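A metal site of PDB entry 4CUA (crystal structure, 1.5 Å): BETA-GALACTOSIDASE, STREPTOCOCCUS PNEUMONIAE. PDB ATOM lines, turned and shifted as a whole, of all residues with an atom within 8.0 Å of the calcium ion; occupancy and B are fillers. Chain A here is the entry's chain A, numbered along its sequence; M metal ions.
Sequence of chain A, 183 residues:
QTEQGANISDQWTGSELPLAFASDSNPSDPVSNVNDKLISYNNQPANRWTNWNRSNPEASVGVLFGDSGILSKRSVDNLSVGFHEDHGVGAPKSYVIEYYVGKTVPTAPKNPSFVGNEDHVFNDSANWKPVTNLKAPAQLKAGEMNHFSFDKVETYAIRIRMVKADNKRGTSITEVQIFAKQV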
ATOM      1  N   GLN A  11     -13.332 -11.741  -6.952  1.00  0.00           N
ATOM      2  CA  GLN A  11     -12.409 -11.244  -5.959  1.00  0.00           C
ATOM      3  C   GLN A  11     -12.307 -12.204  -4.786  1.00  0.00           C
ATOM      4  O   GLN A  11     -13.270 -12.857  -4.436  1.00  0.00           O
ATOM      5  CB  GLN A  11     -12.872  -9.932  -5.308  1.00  0.00           C
ATOM      6  CG  GLN A  11     -12.848  -8.743  -6.196  1.00  0.00           C
ATOM      7  CD  GLN A  11     -13.552  -7.577  -5.502  1.00  0.00           C
ATOM      8  OE1 GLN A  11     -13.368  -7.333  -4.315  1.00  0.00           O
ATOM      9  NE2 GLN A  11     -14.283  -6.750  -6.283  1.00  0.00           N
ATOM     10  N   PRO A  30     -17.348   1.943  -9.930  1.00  0.00           N
ATOM     11  CA  PRO A  30     -16.000   1.411 -10.209  1.00  0.00           C
ATOM     12  C   PRO A  30     -16.060  -0.008 -10.741  1.00  0.00           C
ATOM     13  O   PRO A  30     -17.002  -0.758 -10.439  1.00  0.00           O
ATOM     14  CB  PRO A  30     -15.333   1.414  -8.853  1.00  0.00           C
ATOM     15  CG  PRO A  30     -16.484   1.386  -7.889  1.00  0.00           C
ATOM     16  CD  PRO A  30     -17.540   2.222  -8.527  1.00  0.00           C
ATOM     17  N   VAL A  31     -15.080  -0.403 -11.522  1.00  0.00           N
ATOM     18  CA  VAL A  31     -15.069  -1.729 -12.157  1.00  0.00           C
ATOM     19  C   VAL A  31     -14.922  -2.850 -11.176  1.00  0.00           C
ATOM     20  O   VAL A  31     -15.277  -3.957 -11.495  1.00  0.00           O
ATOM     21  CB  VAL A  31     -13.995  -1.763 -13.278  1.00  0.00           C
ATOM     22  CG1 VAL A  31     -12.610  -1.881 -12.694  1.00  0.00           C
ATOM     23  CG2 VAL A  31     -14.300  -2.898 -14.278  1.00  0.00           C
ATOM     24  N   SER A  32     -14.405  -2.584  -9.999  1.00  0.00           N
ATOM     25  CA  SER A  32     -14.366  -3.601  -8.923  1.00  0.00           C
ATOM     26  C   SER A  32     -15.757  -4.145  -8.632  1.00  0.00           C
ATOM     27  O   SER A  32     -15.923  -5.265  -8.160  1.00  0.00           O
ATOM     28  CB  SER A  32     -13.733  -2.975  -7.645  1.00  0.00           C
ATOM     29  OG  SER A  32     -14.415  -1.797  -7.288  1.00  0.00           O
ATOM     30  N   ASN A  33     -16.814  -3.396  -8.960  1.00  0.00           N
ATOM     31  CA  ASN A  33     -18.157  -3.946  -8.878  1.00  0.00           C
ATOM     32  C   ASN A  33     -18.465  -5.119  -9.712  1.00  0.00           C
ATOM     33  O   ASN A  33     -19.463  -5.773  -9.500  1.00  0.00           O
ATOM     34  CB  ASN A  33     -19.189  -2.870  -9.197  1.00  0.00           C
ATOM     35  CG  ASN A  33     -19.311  -1.807  -8.092  1.00  0.00           C
ATOM     36  OD1 ASN A  33     -18.988  -2.051  -6.922  1.00  0.00           O
ATOM     37  ND2 ASN A  33     -19.846  -0.680  -8.447  1.00  0.00           N
ATOM     38  N   VAL A  34     -17.668  -5.420 -10.746  1.00  0.00           N
ATOM     39  CA  VAL A  34     -18.044  -6.493 -11.643  1.00  0.00           C
ATOM     40  C   VAL A  34     -17.591  -7.909 -11.184  1.00  0.00           C
ATOM     41  O   VAL A  34     -17.933  -8.874 -11.838  1.00  0.00           O
ATOM     42  CB  VAL A  34     -17.651  -6.310 -13.116  1.00  0.00           C
ATOM     43  CG1 VAL A  34     -18.092  -4.921 -13.623  1.00  0.00           C
ATOM     44  CG2 VAL A  34     -16.140  -6.528 -13.354  1.00  0.00           C
ATOM     45  N   ASN A  35     -16.779  -7.968 -10.137  1.00  0.00           N
ATOM     46  CA  ASN A  35     -16.356  -9.294  -9.666  1.00  0.00           C
ATOM     47  C   ASN A  35     -16.415  -9.343  -8.187  1.00  0.00           C
ATOM     48  O   ASN A  35     -15.600 -10.066  -7.519  1.00  0.00           O
ATOM     49  CB  ASN A  35     -14.945  -9.667 -10.181  1.00  0.00           C
ATOM     50  CG  ASN A  35     -13.852  -8.805  -9.618  1.00  0.00           C
ATOM     51  OD1 ASN A  35     -14.029  -7.700  -9.183  1.00  0.00           O
ATOM     52  ND2 ASN A  35     -12.606  -9.381  -9.691  1.00  0.00           N
ATOM     53  N   ASP A  36     -17.451  -8.700  -7.612  1.00  0.00           N
ATOM     54  CA  ASP A  36     -17.635  -8.599  -6.166  1.00  0.00           C
ATOM     55  C   ASP A  36     -18.658  -9.628  -5.616  1.00  0.00           C
ATOM     56  O   ASP A  36     -18.958  -9.610  -4.396  1.00  0.00           O
ATOM     57  CB  ASP A  36     -17.967  -7.216  -5.713  1.00  0.00           C
ATOM     58  CG  ASP A  36     -19.282  -6.710  -6.228  1.00  0.00           C
ATOM     59  OD1 ASP A  36     -19.971  -7.406  -6.947  1.00  0.00           O
ATOM     60  OD2 ASP A  36     -19.576  -5.550  -5.905  1.00  0.00           O
ATOM     61  N   LYS A  37     -19.178 -10.470  -6.490  1.00  0.00           N
ATOM     62  CA  LYS A  37     -20.150 -11.536  -6.176  1.00  0.00           C
ATOM     63  C   LYS A  37     -21.491 -10.967  -5.834  1.00  0.00           C
ATOM     64  O   LYS A  37     -22.377 -11.731  -5.419  1.00  0.00           O
ATOM     65  CB  LYS A  37     -19.637 -12.500  -5.070  1.00  0.00           C
ATOM     66  CG  LYS A  37     -18.388 -13.289  -5.554  1.00  0.00           C
ATOM     67  CD  LYS A  37     -17.656 -13.882  -4.375  1.00  0.00           C
ATOM     68  CE  LYS A  37     -16.762 -12.808  -3.725  1.00  0.00           C
ATOM     69  NZ  LYS A  37     -15.944 -13.229  -2.570  1.00  0.00           N
ATOM     70  N   LEU A  38     -21.731  -9.684  -6.039  1.00  0.00           N
ATOM     71  CA  LEU A  38     -23.067  -9.085  -5.868  1.00  0.00           C
ATOM     72  C   LEU A  38     -23.616  -8.881  -7.270  1.00  0.00           C
ATOM     73  O   LEU A  38     -22.918  -8.421  -8.161  1.00  0.00           O
ATOM     74  CB  LEU A  38     -23.002  -7.750  -5.149  1.00  0.00           C
ATOM     75  CG  LEU A  38     -22.482  -7.804  -3.733  1.00  0.00           C
ATOM     76  CD1 LEU A  38     -22.401  -6.411  -3.144  1.00  0.00           C
ATOM     77  CD2 LEU A  38     -23.334  -8.750  -2.868  1.00  0.00           C
ATOM     78  N   ILE A  39     -24.842  -9.276  -7.493  1.00  0.00           N
ATOM     79  CA  ILE A  39     -25.494  -9.163  -8.773  1.00  0.00           C
ATOM     80  C   ILE A  39     -26.753  -8.394  -8.546  1.00  0.00           C
ATOM     81  O   ILE A  39     -27.647  -8.826  -7.782  1.00  0.00           O
ATOM     82  CB  ILE A  39     -25.806 -10.514  -9.408  1.00  0.00           C
ATOM     83  CG1 ILE A  39     -24.480 -11.318  -9.583  1.00  0.00           C
ATOM     84  CG2 ILE A  39     -26.563 -10.347 -10.711  1.00  0.00           C
ATOM     85  CD1 ILE A  39     -24.650 -12.598 -10.326  1.00  0.00           C
ATOM     86  N   SER A  40     -26.884  -7.231  -9.183  1.00  0.00           N
ATOM     87  CA  SER A  40     -28.082  -6.401  -9.028  1.00  0.00           C
ATOM     88  C   SER A  40     -28.437  -5.751 -10.353  1.00  0.00           C
ATOM     89  O   SER A  40     -27.629  -5.103 -10.998  1.00  0.00           O
ATOM     90  CB  SER A  40     -27.886  -5.306  -8.017  1.00  0.00           C
ATOM     91  OG  SER A  40     -29.092  -4.523  -8.011  1.00  0.00           O
ATOM     92  N   ALA A  46     -27.716  -0.455  -6.026  1.00  0.00           N
ATOM     93  CA  ALA A  46     -26.973  -0.218  -7.228  1.00  0.00           C
ATOM     94  C   ALA A  46     -25.638  -0.904  -7.089  1.00  0.00           C
ATOM     95  O   ALA A  46     -24.881  -0.652  -6.131  1.00  0.00           O
ATOM     96  CB  ALA A  46     -26.786   1.250  -7.506  1.00  0.00           C
ATOM     97  N   ASN A  47     -25.338  -1.773  -8.045  1.00  0.00           N
ATOM     98  CA  ASN A  47     -24.056  -2.477  -8.046  1.00  0.00           C
ATOM     99  C   ASN A  47     -23.654  -2.778  -9.507  1.00  0.00           C
ATOM    100  O   ASN A  47     -24.236  -3.624 -10.160  1.00  0.00           O
ATOM    101  CB  ASN A  47     -24.153  -3.810  -7.299  1.00  0.00           C
ATOM    102  CG  ASN A  47     -22.816  -4.521  -7.257  1.00  0.00           C
ATOM    103  OD1 ASN A  47     -22.512  -5.353  -8.132  1.00  0.00           O
ATOM    104  ND2 ASN A  47     -22.006  -4.182  -6.297  1.00  0.00           N
ATOM    105  N   ARG A  48     -22.772  -1.972 -10.036  1.00  0.00           N
ATOM    106  CA  ARG A  48     -22.444  -2.049 -11.446  1.00  0.00           C
ATOM    107  C   ARG A  48     -21.216  -1.256 -11.777  1.00  0.00           C
ATOM    108  O   ARG A  48     -20.919  -0.269 -11.101  1.00  0.00           O
ATOM    109  CB  ARG A  48     -23.631  -1.615 -12.284  1.00  0.00           C
ATOM    110  CG  ARG A  48     -24.192  -0.251 -11.895  1.00  0.00           C
ATOM    111  CD  ARG A  48     -25.348   0.105 -12.786  1.00  0.00           C
ATOM    112  NE  ARG A  48     -25.998   1.363 -12.425  1.00  0.00           N
ATOM    113  CZ  ARG A  48     -27.009   1.480 -11.575  1.00  0.00           C
ATOM    114  NH1 ARG A  48     -27.494   0.466 -10.896  1.00  0.00           N
ATOM    115  NH2 ARG A  48     -27.518   2.698 -11.338  1.00  0.00           N
ATOM    116  N   TRP A  49     -20.472  -1.696 -12.826  1.00  0.00           N
ATOM    117  CA  TRP A  49     -19.614  -0.815 -13.557  1.00  0.00           C
ATOM    118  C   TRP A  49     -20.448  -0.172 -14.648  1.00  0.00           C
ATOM    119  O   TRP A  49     -21.303  -0.805 -15.254  1.00  0.00           O
ATOM    120  CB  TRP A  49     -18.492  -1.591 -14.228  1.00  0.00           C
ATOM    121  CG  TRP A  49     -17.763  -0.759 -15.247  1.00  0.00           C
ATOM    122  CD1 TRP A  49     -16.725   0.036 -15.025  1.00  0.00           C
ATOM    123  CD2 TRP A  49     -18.059  -0.664 -16.659  1.00  0.00           C
ATOM    124  NE1 TRP A  49     -16.321   0.639 -16.187  1.00  0.00           N
ATOM    125  CE2 TRP A  49     -17.150   0.252 -17.199  1.00  0.00           C
ATOM    126  CE3 TRP A  49     -19.020  -1.241 -17.476  1.00  0.00           C
ATOM    127  CZ2 TRP A  49     -17.131   0.569 -18.562  1.00  0.00           C
ATOM    128  CZ3 TRP A  49     -18.987  -0.921 -18.838  1.00  0.00           C
ATOM    129  CH2 TRP A  49     -18.058  -0.018 -19.344  1.00  0.00           C
ATOM    130  N   GLY A  82     -23.352 -10.006 -16.993  1.00  0.00           N
ATOM    131  CA  GLY A  82     -24.679  -9.552 -16.613  1.00  0.00           C
ATOM    132  C   GLY A  82     -24.837  -8.082 -16.948  1.00  0.00           C
ATOM    133  O   GLY A  82     -24.416  -7.228 -16.188  1.00  0.00           O
ATOM    134  N   ILE A 173     -22.642  -3.087 -16.567  1.00  0.00           N
ATOM    135  CA  ILE A 173     -22.419  -4.486 -16.175  1.00  0.00           C
ATOM    136  C   ILE A 173     -22.490  -4.597 -14.658  1.00  0.00           C
ATOM    137  O   ILE A 173     -21.723  -3.970 -13.964  1.00  0.00           O
ATOM    138  CB  ILE A 173     -21.055  -4.961 -16.643  1.00  0.00           C
ATOM    139  CG1 ILE A 173     -20.962  -5.006 -18.168  1.00  0.00           C
ATOM    140  CG2 ILE A 173     -20.750  -6.366 -16.076  1.00  0.00           C
ATOM    141  CD1 ILE A 173     -19.541  -5.234 -18.681  1.00  0.00           C
ATOM    142  N   THR A 174     -23.383  -5.489 -14.171  1.00  0.00           N
ATOM    143  CA  THR A 174     -23.425  -5.730 -12.706  1.00  0.00           C
ATOM    144  C   THR A 174     -22.373  -6.777 -12.240  1.00  0.00           C
ATOM    145  O   THR A 174     -21.841  -6.645 -11.174  1.00  0.00           O
ATOM    146  CB  THR A 174     -24.802  -6.086 -12.216  1.00  0.00           C
ATOM    147  OG1 THR A 174     -24.747  -6.284 -10.793  1.00  0.00           O
ATOM    148  CG2 THR A 174     -25.418  -7.255 -12.869  1.00  0.00           C
ATOM    149  N   GLU A 175     -22.070  -7.734 -13.107  1.00  0.00           N
ATOM    150  CA  GLU A 175     -21.123  -8.811 -12.746  1.00  0.00           C
ATOM    151  C   GLU A 175     -20.673  -9.485 -13.999  1.00  0.00           C
ATOM    152  O   GLU A 175     -21.447  -9.656 -14.919  1.00  0.00           O
ATOM    153  CB  GLU A 175     -21.819  -9.811 -11.793  1.00  0.00           C
ATOM    154  CG  GLU A 175     -20.897 -10.758 -11.037  1.00  0.00           C
ATOM    155  CD  GLU A 175     -20.082 -10.164  -9.937  1.00  0.00           C
ATOM    156  OE1 GLU A 175     -20.164  -8.959  -9.642  1.00  0.00           O
ATOM    157  OE2 GLU A 175     -19.292 -10.939  -9.274  1.00  0.00           O
ATOM    158  N   VAL A 176     -19.398  -9.925 -13.962  1.00  0.00           N
ATOM    159  CA  VAL A 176     -18.894 -10.881 -14.930  1.00  0.00           C
ATOM    160  C   VAL A 176     -18.507 -12.128 -14.183  1.00  0.00           C
ATOM    161  O   VAL A 176     -18.246 -12.063 -12.979  1.00  0.00           O
ATOM    162  CB  VAL A 176     -17.692 -10.375 -15.723  1.00  0.00           C
ATOM    163  CG1 VAL A 176     -18.037  -9.035 -16.383  1.00  0.00           C
ATOM    164  CG2 VAL A 176     -16.442 -10.249 -14.847  1.00  0.00           C
HETATM  165 CA    CA M   1     -21.244  -7.061  -8.940  1.00  0.00          CA
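The backbone carbonyl oxygen (O) of Asn 33 is bound to the calcium ion (2.3 Å).
The side-chain amide oxygen (OD1) of Asn 47 is bound to the calcium ion (2.3 Å).
The backbone carbonyl oxygen (O) of Leu 38 is bound to the calcium ion, at 2.3 Å.
The calcium ion is bound by the side-chain carboxylate (OE1) of Glu 175 (2.3 Å).
The calcium ion is bound by the backbone carbonyl oxygen (O) of Thr 174 (2.3 Å).
The calcium ion is bound by the side-chain carboxylate (OD1) of Asp 36 (2.4 Å).
The calcium ion has six donor atoms within binding distance.
O of Glu 175 lies within hydrogen-bond range of N of Gly 82 (2.8 Å).
ND2 of Asn 33 lies within hydrogen-bond range of O of Arg 48, at 2.9 Å.
The backbone NH (N) of Ser 40 sits at hydrogen-bond distance from the side-chain hydroxyl (OG1) of Thr 174, at 2.8 Å.
N of Thr 174 lies within hydrogen-bond range of O of Gly 82, 2.9 Å away.
The backbone carbonyl oxygen (O) of Pro 30 lies close to the side-chain amide nitrogen (ND2) of Asn 33 (3.5 Å).
The backbone NH (N) of Lys 37 sits at hydrogen-bond distance from the side-chain carboxylate (OE2) of Glu 175.
Six residues have an atom within 4 Å of the calcium ion: Asn 33, Asp 36, Leu 38, Asn 47, Thr 174 and Glu 175.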
